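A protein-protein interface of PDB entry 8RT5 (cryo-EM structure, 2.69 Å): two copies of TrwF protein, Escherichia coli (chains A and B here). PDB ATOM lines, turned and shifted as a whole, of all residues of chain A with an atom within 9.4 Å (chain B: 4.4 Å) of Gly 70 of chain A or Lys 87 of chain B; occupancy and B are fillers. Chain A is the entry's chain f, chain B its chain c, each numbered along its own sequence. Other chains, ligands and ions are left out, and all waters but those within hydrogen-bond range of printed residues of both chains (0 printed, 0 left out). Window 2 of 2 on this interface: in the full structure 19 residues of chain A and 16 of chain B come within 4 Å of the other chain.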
ATOM      1  N   HIS A  67      -1.421  -5.191  11.698  1.00  0.00           N
ATOM      2  CA  HIS A  67      -0.386  -5.110  10.686  1.00  0.00           C
ATOM      3  C   HIS A  67      -0.825  -5.941   9.492  1.00  0.00           C
ATOM      4  O   HIS A  67      -1.754  -6.744   9.574  1.00  0.00           O
ATOM      5  CB  HIS A  67       0.969  -5.581  11.220  1.00  0.00           C
ATOM      6  CG  HIS A  67       1.091  -7.066  11.326  1.00  0.00           C
ATOM      7  ND1 HIS A  67       0.494  -7.787  12.333  1.00  0.00           N
ATOM      8  CD2 HIS A  67       1.730  -7.965  10.545  1.00  0.00           C
ATOM      9  CE1 HIS A  67       0.763  -9.068  12.171  1.00  0.00           C
ATOM     10  NE2 HIS A  67       1.511  -9.203  11.093  1.00  0.00           N
ATOM     11  N   ALA A  68      -0.151  -5.733   8.368  1.00  0.00           N
ATOM     12  CA  ALA A  68      -0.413  -6.524   7.173  1.00  0.00           C
ATOM     13  C   ALA A  68       0.889  -6.687   6.416  1.00  0.00           C
ATOM     14  O   ALA A  68       1.601  -5.707   6.191  1.00  0.00           O
ATOM     15  CB  ALA A  68      -1.465  -5.869   6.291  1.00  0.00           C
ATOM     16  N   PHE A  69       1.204  -7.914   6.043  1.00  0.00           N
ATOM     17  CA  PHE A  69       2.299  -8.170   5.128  1.00  0.00           C
ATOM     18  C   PHE A  69       1.758  -8.340   3.720  1.00  0.00           C
ATOM     19  O   PHE A  69       0.692  -8.914   3.504  1.00  0.00           O
ATOM     20  CB  PHE A  69       3.069  -9.425   5.531  1.00  0.00           C
ATOM     21  CG  PHE A  69       4.079  -9.201   6.604  1.00  0.00           C
ATOM     22  CD1 PHE A  69       5.317  -8.675   6.301  1.00  0.00           C
ATOM     23  CD2 PHE A  69       3.797  -9.531   7.914  1.00  0.00           C
ATOM     24  CE1 PHE A  69       6.248  -8.475   7.284  1.00  0.00           C
ATOM     25  CE2 PHE A  69       4.727  -9.333   8.896  1.00  0.00           C
ATOM     26  CZ  PHE A  69       5.955  -8.806   8.583  1.00  0.00           C
ATOM     27  N   GLY A  70       2.510  -7.825   2.752  1.00  0.00           N
ATOM     28  CA  GLY A  70       2.216  -8.153   1.371  1.00  0.00           C
ATOM     29  C   GLY A  70       2.486  -9.613   1.074  1.00  0.00           C
ATOM     30  O   GLY A  70       1.987 -10.158   0.090  1.00  0.00           O
ATOM     31  N   ASP A  71       3.305 -10.254   1.904  1.00  0.00           N
ATOM     32  CA  ASP A  71       3.574 -11.685   1.835  1.00  0.00           C
ATOM     33  C   ASP A  71       3.915 -12.158   3.239  1.00  0.00           C
ATOM     34  O   ASP A  71       5.030 -11.931   3.715  1.00  0.00           O
ATOM     35  CB  ASP A  71       4.719 -11.981   0.864  1.00  0.00           C
ATOM     36  CG  ASP A  71       5.003 -13.463   0.719  1.00  0.00           C
ATOM     37  OD1 ASP A  71       5.880 -13.811  -0.091  1.00  0.00           O
ATOM     38  OD2 ASP A  71       4.347 -14.285   1.387  1.00  0.00           O
ATOM     39  N   SER A  72       2.963 -12.824   3.896  1.00  0.00           N
ATOM     40  CA  SER A  72       3.145 -13.211   5.290  1.00  0.00           C
ATOM     41  C   SER A  72       4.205 -14.282   5.479  1.00  0.00           C
ATOM     42  O   SER A  72       4.921 -14.249   6.482  1.00  0.00           O
ATOM     43  CB  SER A  72       1.831 -13.709   5.881  1.00  0.00           C
ATOM     44  OG  SER A  72       0.914 -12.649   6.024  1.00  0.00           O
ATOM     45  N   GLU A  73       4.313 -15.236   4.560  1.00  0.00           N
ATOM     46  CA  GLU A  73       5.269 -16.322   4.707  1.00  0.00           C
ATOM     47  C   GLU A  73       6.699 -15.907   4.412  1.00  0.00           C
ATOM     48  O   GLU A  73       7.616 -16.698   4.651  1.00  0.00           O
ATOM     49  CB  GLU A  73       4.888 -17.492   3.800  1.00  0.00           C
ATOM     50  CG  GLU A  73       3.410 -17.770   3.766  1.00  0.00           C
ATOM     51  CD  GLU A  73       3.071 -19.035   3.015  1.00  0.00           C
ATOM     52  OE1 GLU A  73       1.960 -19.568   3.217  1.00  0.00           O
ATOM     53  OE2 GLU A  73       3.915 -19.500   2.221  1.00  0.00           O
ATOM     54  N   ALA A  74       6.913 -14.704   3.893  1.00  0.00           N
ATOM     55  CA  ALA A  74       8.269 -14.242   3.641  1.00  0.00           C
ATOM     56  C   ALA A  74       8.971 -13.793   4.916  1.00  0.00           C
ATOM     57  O   ALA A  74      10.197 -13.877   5.002  1.00  0.00           O
ATOM     58  CB  ALA A  74       8.254 -13.104   2.624  1.00  0.00           C
ATOM     59  N   TYR A  75       8.224 -13.322   5.908  1.00  0.00           N
ATOM     60  CA  TYR A  75       8.796 -12.755   7.115  1.00  0.00           C
ATOM     61  C   TYR A  75       8.113 -13.324   8.345  1.00  0.00           C
ATOM     62  O   TYR A  75       6.958 -13.750   8.292  1.00  0.00           O
ATOM     63  CB  TYR A  75       8.673 -11.238   7.121  1.00  0.00           C
ATOM     64  CG  TYR A  75       9.648 -10.573   6.200  1.00  0.00           C
ATOM     65  CD1 TYR A  75       9.369 -10.433   4.856  1.00  0.00           C
ATOM     66  CD2 TYR A  75      10.854 -10.091   6.669  1.00  0.00           C
ATOM     67  CE1 TYR A  75      10.257  -9.836   4.009  1.00  0.00           C
ATOM     68  CE2 TYR A  75      11.750  -9.492   5.827  1.00  0.00           C
ATOM     69  CZ  TYR A  75      11.446  -9.365   4.495  1.00  0.00           C
ATOM     70  OH  TYR A  75      12.333  -8.763   3.644  1.00  0.00           O
ATOM     71  N   ALA A  93      12.574 -12.589  -0.265  1.00  0.00           N
ATOM     72  CA  ALA A  93      11.509 -12.063   0.587  1.00  0.00           C
ATOM     73  C   ALA A  93      11.419 -10.554   0.391  1.00  0.00           C
ATOM     74  O   ALA A  93      11.885  -9.755   1.201  1.00  0.00           O
ATOM     75  CB  ALA A  93      11.759 -12.433   2.041  1.00  0.00           C
ATOM     76  N   ASN A  94      10.796 -10.164  -0.715  1.00  0.00           N
ATOM     77  CA  ASN A  94      10.617  -8.764  -1.080  1.00  0.00           C
ATOM     78  C   ASN A  94       9.131  -8.449  -1.031  1.00  0.00           C
ATOM     79  O   ASN A  94       8.368  -8.897  -1.891  1.00  0.00           O
ATOM     80  CB  ASN A  94      11.193  -8.491  -2.464  1.00  0.00           C
ATOM     81  CG  ASN A  94      12.679  -8.717  -2.521  1.00  0.00           C
ATOM     82  OD1 ASN A  94      13.144  -9.839  -2.697  1.00  0.00           O
ATOM     83  ND2 ASN A  94      13.438  -7.649  -2.372  1.00  0.00           N
ATOM     84  N   THR A  95       8.720  -7.684  -0.027  1.00  0.00           N
ATOM     85  CA  THR A  95       7.309  -7.399   0.193  1.00  0.00           C
ATOM     86  C   THR A  95       7.203  -6.040   0.877  1.00  0.00           C
ATOM     87  O   THR A  95       8.142  -5.240   0.872  1.00  0.00           O
ATOM     88  CB  THR A  95       6.658  -8.539   0.988  1.00  0.00           C
ATOM     89  OG1 THR A  95       5.248  -8.331   1.049  1.00  0.00           O
ATOM     90  CG2 THR A  95       7.209  -8.604   2.394  1.00  0.00           C
ATOM     91  N   ASN A  96       6.042  -5.756   1.455  1.00  0.00           N
ATOM     92  CA  ASN A  96       5.836  -4.538   2.218  1.00  0.00           C
ATOM     93  C   ASN A  96       5.164  -4.881   3.536  1.00  0.00           C
ATOM     94  O   ASN A  96       4.541  -5.933   3.679  1.00  0.00           O
ATOM     95  CB  ASN A  96       5.006  -3.504   1.441  1.00  0.00           C
ATOM     96  CG  ASN A  96       3.540  -3.873   1.342  1.00  0.00           C
ATOM     97  OD1 ASN A  96       3.187  -5.029   1.135  1.00  0.00           O
ATOM     98  ND2 ASN A  96       2.675  -2.884   1.493  1.00  0.00           N
ATOM     99  N   LEU A  97       5.318  -3.987   4.504  1.00  0.00           N
ATOM    100  CA  LEU A  97       4.703  -4.128   5.812  1.00  0.00           C
ATOM    101  C   LEU A  97       4.029  -2.818   6.179  1.00  0.00           C
ATOM    102  O   LEU A  97       4.622  -1.748   6.026  1.00  0.00           O
ATOM    103  CB  LEU A  97       5.741  -4.509   6.867  1.00  0.00           C
ATOM    104  CG  LEU A  97       5.310  -4.539   8.330  1.00  0.00           C
ATOM    105  CD1 LEU A  97       4.210  -5.555   8.556  1.00  0.00           C
ATOM    106  CD2 LEU A  97       6.498  -4.832   9.207  1.00  0.00           C
ATOM    107  N   ILE A  98       2.791  -2.905   6.655  1.00  0.00           N
ATOM    108  CA  ILE A  98       2.041  -1.748   7.136  1.00  0.00           C
ATOM    109  C   ILE A  98       1.604  -2.086   8.557  1.00  0.00           C
ATOM    110  O   ILE A  98       0.936  -3.094   8.793  1.00  0.00           O
ATOM    111  CB  ILE A  98       0.838  -1.408   6.253  1.00  0.00           C
ATOM    112  CG1 ILE A  98       1.280  -1.188   4.809  1.00  0.00           C
ATOM    113  CG2 ILE A  98       0.125  -0.181   6.777  1.00  0.00           C
ATOM    114  CD1 ILE A  98       0.149  -1.123   3.839  1.00  0.00           C
ATOM    115  N   PHE A 108       6.541   0.215   5.465  1.00  0.00           N
ATOM    116  CA  PHE A 108       7.875  -0.327   5.286  1.00  0.00           C
ATOM    117  C   PHE A 108       7.957  -1.085   3.974  1.00  0.00           C
ATOM    118  O   PHE A 108       7.077  -1.882   3.647  1.00  0.00           O
ATOM    119  CB  PHE A 108       8.247  -1.274   6.427  1.00  0.00           C
ATOM    120  CG  PHE A 108       8.130  -0.665   7.783  1.00  0.00           C
ATOM    121  CD1 PHE A 108       9.091   0.208   8.244  1.00  0.00           C
ATOM    122  CD2 PHE A 108       7.070  -0.981   8.603  1.00  0.00           C
ATOM    123  CE1 PHE A 108       8.988   0.760   9.488  1.00  0.00           C
ATOM    124  CE2 PHE A 108       6.967  -0.430   9.849  1.00  0.00           C
ATOM    125  CZ  PHE A 108       7.924   0.442  10.292  1.00  0.00           C
ATOM    126  N   ARG A 109       9.030  -0.849   3.228  1.00  0.00           N
ATOM    127  CA  ARG A 109       9.311  -1.623   2.024  1.00  0.00           C
ATOM    128  C   ARG A 109      10.429  -2.589   2.397  1.00  0.00           C
ATOM    129  O   ARG A 109      11.584  -2.195   2.561  1.00  0.00           O
ATOM    130  CB  ARG A 109       9.693  -0.755   0.854  1.00  0.00           C
ATOM    131  CG  ARG A 109      10.354  -1.544  -0.245  1.00  0.00           C
ATOM    132  CD  ARG A 109      10.198  -0.887  -1.584  1.00  0.00           C
ATOM    133  NE  ARG A 109      11.137  -1.446  -2.545  1.00  0.00           N
ATOM    134  CZ  ARG A 109      12.169  -0.790  -3.055  1.00  0.00           C
ATOM    135  NH1 ARG A 109      12.965  -1.388  -3.926  1.00  0.00           N
ATOM    136  NH2 ARG A 109      12.413   0.452  -2.684  1.00  0.00           N
ATOM    137  N   LEU A 110      10.075  -3.858   2.554  1.00  0.00           N
ATOM    138  CA  LEU A 110      11.022  -4.875   2.992  1.00  0.00           C
ATOM    139  C   LEU A 110      11.727  -5.468   1.782  1.00  0.00           C
ATOM    140  O   LEU A 110      11.093  -6.105   0.938  1.00  0.00           O
ATOM    141  CB  LEU A 110      10.292  -5.954   3.781  1.00  0.00           C
ATOM    142  CG  LEU A 110       9.468  -5.450   4.958  1.00  0.00           C
ATOM    143  CD1 LEU A 110       8.729  -6.586   5.619  1.00  0.00           C
ATOM    144  CD2 LEU A 110      10.361  -4.751   5.947  1.00  0.00           C
ATOM    145  N   GLY B  51       2.444  -9.445  -4.260  1.00  0.00           N
ATOM    146  CA  GLY B  51       3.129  -9.391  -2.988  1.00  0.00           C
ATOM    147  C   GLY B  51       3.057  -8.073  -2.261  1.00  0.00           C
ATOM    148  O   GLY B  51       3.903  -7.817  -1.400  1.00  0.00           O
ATOM    149  N   VAL B  52       2.092  -7.220  -2.583  1.00  0.00           N
ATOM    150  CA  VAL B  52       1.932  -5.936  -1.921  1.00  0.00           C
ATOM    151  C   VAL B  52       0.525  -5.827  -1.358  1.00  0.00           C
ATOM    152  O   VAL B  52      -0.470  -6.060  -2.045  1.00  0.00           O
ATOM    153  CB  VAL B  52       2.238  -4.757  -2.861  1.00  0.00           C
ATOM    154  CG1 VAL B  52       1.910  -3.448  -2.192  1.00  0.00           C
ATOM    155  CG2 VAL B  52       3.696  -4.782  -3.240  1.00  0.00           C
ATOM    156  N   ALA B  53       0.456  -5.459  -0.086  1.00  0.00           N
ATOM    157  CA  ALA B  53      -0.796  -5.184   0.593  1.00  0.00           C
ATOM    158  C   ALA B  53      -1.095  -3.699   0.472  1.00  0.00           C
ATOM    159  O   ALA B  53      -0.197  -2.869   0.617  1.00  0.00           O
ATOM    160  CB  ALA B  53      -0.729  -5.597   2.062  1.00  0.00           C
ATOM    161  N   ALA B  74      -9.781 -13.849  -5.792  1.00  0.00           N
ATOM    162  CA  ALA B  74      -8.696 -13.092  -6.395  1.00  0.00           C
ATOM    163  C   ALA B  74      -7.948 -12.245  -5.375  1.00  0.00           C
ATOM    164  O   ALA B  74      -6.759 -11.977  -5.556  1.00  0.00           O
ATOM    165  CB  ALA B  74      -9.235 -12.209  -7.518  1.00  0.00           C
ATOM    166  N   TYR B  75      -8.615 -11.818  -4.309  1.00  0.00           N
ATOM    167  CA  TYR B  75      -8.036 -10.906  -3.340  1.00  0.00           C
ATOM    168  C   TYR B  75      -8.287 -11.402  -1.928  1.00  0.00           C
ATOM    169  O   TYR B  75      -9.249 -12.126  -1.668  1.00  0.00           O
ATOM    170  CB  TYR B  75      -8.609  -9.505  -3.496  1.00  0.00           C
ATOM    171  CG  TYR B  75      -8.059  -8.781  -4.686  1.00  0.00           C
ATOM    172  CD1 TYR B  75      -8.601  -8.971  -5.941  1.00  0.00           C
ATOM    173  CD2 TYR B  75      -6.992  -7.914  -4.560  1.00  0.00           C
ATOM    174  CE1 TYR B  75      -8.100  -8.323  -7.032  1.00  0.00           C
ATOM    175  CE2 TYR B  75      -6.483  -7.261  -5.649  1.00  0.00           C
ATOM    176  CZ  TYR B  75      -7.043  -7.468  -6.885  1.00  0.00           C
ATOM    177  OH  TYR B  75      -6.544  -6.816  -7.981  1.00  0.00           O
ATOM    178  N   ALA B  76      -7.404 -11.011  -1.018  1.00  0.00           N
ATOM    179  CA  ALA B  76      -7.584 -11.237   0.406  1.00  0.00           C
ATOM    180  C   ALA B  76      -8.073  -9.948   1.042  1.00  0.00           C
ATOM    181  O   ALA B  76      -7.607  -8.862   0.690  1.00  0.00           O
ATOM    182  CB  ALA B  76      -6.289 -11.695   1.072  1.00  0.00           C
ATOM    183  N   ILE B  86      -6.099  -5.092   1.380  1.00  0.00           N
ATOM    184  CA  ILE B  86      -6.378  -5.997   0.276  1.00  0.00           C
ATOM    185  C   ILE B  86      -5.060  -6.413  -0.355  1.00  0.00           C
ATOM    186  O   ILE B  86      -4.050  -5.715  -0.268  1.00  0.00           O
ATOM    187  CB  ILE B  86      -7.316  -5.389  -0.788  1.00  0.00           C
ATOM    188  CG1 ILE B  86      -6.724  -4.109  -1.363  1.00  0.00           C
ATOM    189  CG2 ILE B  86      -8.689  -5.146  -0.205  1.00  0.00           C
ATOM    190  CD1 ILE B  86      -7.436  -3.624  -2.576  1.00  0.00           C
ATOM    191  N   LYS B  87      -5.090  -7.567  -0.993  1.00  0.00           N
ATOM    192  CA  LYS B  87      -3.894  -8.259  -1.440  1.00  0.00           C
ATOM    193  C   LYS B  87      -4.279  -9.340  -2.436  1.00  0.00           C
ATOM    194  O   LYS B  87      -5.121 -10.189  -2.128  1.00  0.00           O
ATOM    195  CB  LYS B  87      -3.188  -8.800  -0.200  1.00  0.00           C
ATOM    196  CG  LYS B  87      -1.832  -9.438  -0.303  1.00  0.00           C
ATOM    197  CD  LYS B  87      -1.952 -10.926  -0.492  1.00  0.00           C
ATOM    198  CE  LYS B  87      -0.590 -11.563  -0.506  1.00  0.00           C
ATOM    199  NZ  LYS B  87      -0.648 -13.026  -0.719  1.00  0.00           N
ATOM    200  N   PRO B  88      -3.715  -9.333  -3.642  1.00  0.00           N
ATOM    201  CA  PRO B  88      -4.091 -10.350  -4.632  1.00  0.00           C
ATOM    202  C   PRO B  88      -3.685 -11.751  -4.197  1.00  0.00           C
ATOM    203  O   PRO B  88      -2.613 -11.957  -3.628  1.00  0.00           O
ATOM    204  CB  PRO B  88      -3.355  -9.903  -5.900  1.00  0.00           C
ATOM    205  CG  PRO B  88      -2.292  -8.993  -5.435  1.00  0.00           C
ATOM    206  CD  PRO B  88      -2.809  -8.323  -4.209  1.00  0.00           C
ATOM    207  N   GLN B  89      -4.562 -12.714  -4.477  1.00  0.00           N
ATOM    208  CA  GLN B  89      -4.384 -14.122  -4.145  1.00  0.00           C
ATOM    209  C   GLN B  89      -4.264 -15.005  -5.376  1.00  0.00           C
ATOM    210  O   GLN B  89      -4.124 -16.222  -5.244  1.00  0.00           O
ATOM    211  CB  GLN B  89      -5.549 -14.616  -3.287  1.00  0.00           C
ATOM    212  CG  GLN B  89      -5.672 -13.981  -1.935  1.00  0.00           C
ATOM    213  CD  GLN B  89      -4.517 -14.357  -1.043  1.00  0.00           C
ATOM    214  OE1 GLN B  89      -4.061 -15.494  -1.063  1.00  0.00           O
ATOM    215  NE2 GLN B  89      -4.027 -13.409  -0.264  1.00  0.00           N
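Hydrophobic or aromatic side chains of chain B within 4 Å of the printed part of chain A: Val 52 and Ala 53.
Of the 18 printed residues of chain A, 5 touch a printed residue of chain B.
Printed residues of chain A that touch a printed residue of chain B: Phe 69, Gly 70, Thr 95, Asn 96 and Ile 98.
Hydrophobic or aromatic side chains of chain A that line the printed part of chain B: Ile 98.
Among the printed residues, 10 pairs touch across the chains.
Among the printed residues, no Asp or Glu carboxylate lies within 4 Å of a Lys or Arg side-chain nitrogen of the other chain.
Positions printed for both chains: 74 and 75.
The backbone NH (N) of Ala 76 of chain B lies within hydrogen-bond range of the backbone carbonyl oxygen (O) of Lys 87 of chain B (2.7 Å).
The side-chain amide nitrogen (NE2) of Gln 89 of chain B lies close to the side-chain amino group (NZ) of Lys 87 of chain B (3.4 Å).
O of Ile 98 of chain A sits at hydrogen-bond distance from N of Ala 68 of chain A (2.9 Å).
The backbone NH of Gly 70 of chain A lies close to the side-chain hydroxyl of Thr 95 of chain A (3.3 Å).
N of Gly 70 of chain A is in hydrogen-bond range of O of Asn 96 of chain A, at 2.9 Å.
O of Thr 95 of chain A sits at hydrogen-bond distance from N of Leu 110 of chain A (2.9 Å).
Gly 70 of chain A touches four residues of chain B.
Of the printed residues of chain A, Lys 87 of chain B touches Gly 70.
Of chain A, only Gly 70, Thr 95 and Asn 96 come within 4 Å of Gly 51 of chain B.
No residue of chain A comes within 4 Å of Ala 76 of chain B.
Of the printed residues of chain B, Thr 95 of chain A touches Gly 51.
Printed residues of chain B within 4 Å of Ile 98 of chain A: Ala 53 (3.7 Å).
Of the printed residues of chain A, Ala 53 of chain B touches Phe 69, Gly 70, Asn 96 and Ile 98.
Of the printed residues of chain B, Asn 96 of chain A touches Gly 51 (3.8 Å), Val 52 (3.4 Å) and Ala 53 (3.0 Å).
Ala 93 of chain A touches none of the printed residues of chain B.
Phe 108 of chain A touches none of the printed residues of chain B.
The nearest printed residue of chain B that does not touch Gly 70 of chain A is Pro 88 of chain B (6.2 Å).
The nearest printed residue of chain A that does not touch Ala 53 of chain B is Ala 68 of chain A (4.3 Å).
O of Phe 69 of chain A touches CB of Ala 53 of chain B, 3.9 Å away.
Gly 70 of chain A touches Val 52 of chain B (CA to C, 3.96 Å).
N of Ala 53 of chain B touches CA of Gly 70 of chain A (3.5 Å).
Lys 87 of chain B touches Gly 70 of chain A.
OD1 of Asn 96 of chain A touches O of Gly 51 of chain B (3.8 Å).
OD1 of Asn 96 of chain A touches CA of Val 52 of chain B, 3.4 Å away.
Ile 98 of chain A touches Ala 53 of chain B.
OG1 of Thr 95 of chain A lies within hydrogen-bond range of O of Gly 51 of chain B (2.8 Å).
O of Ala 53 of chain B is in hydrogen-bond range of ND2 of Asn 96 of chain A (3.0 Å).
O of Gly 70 of chain A sits close to O of Gly 51 of chain B, at 3.4 Å.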
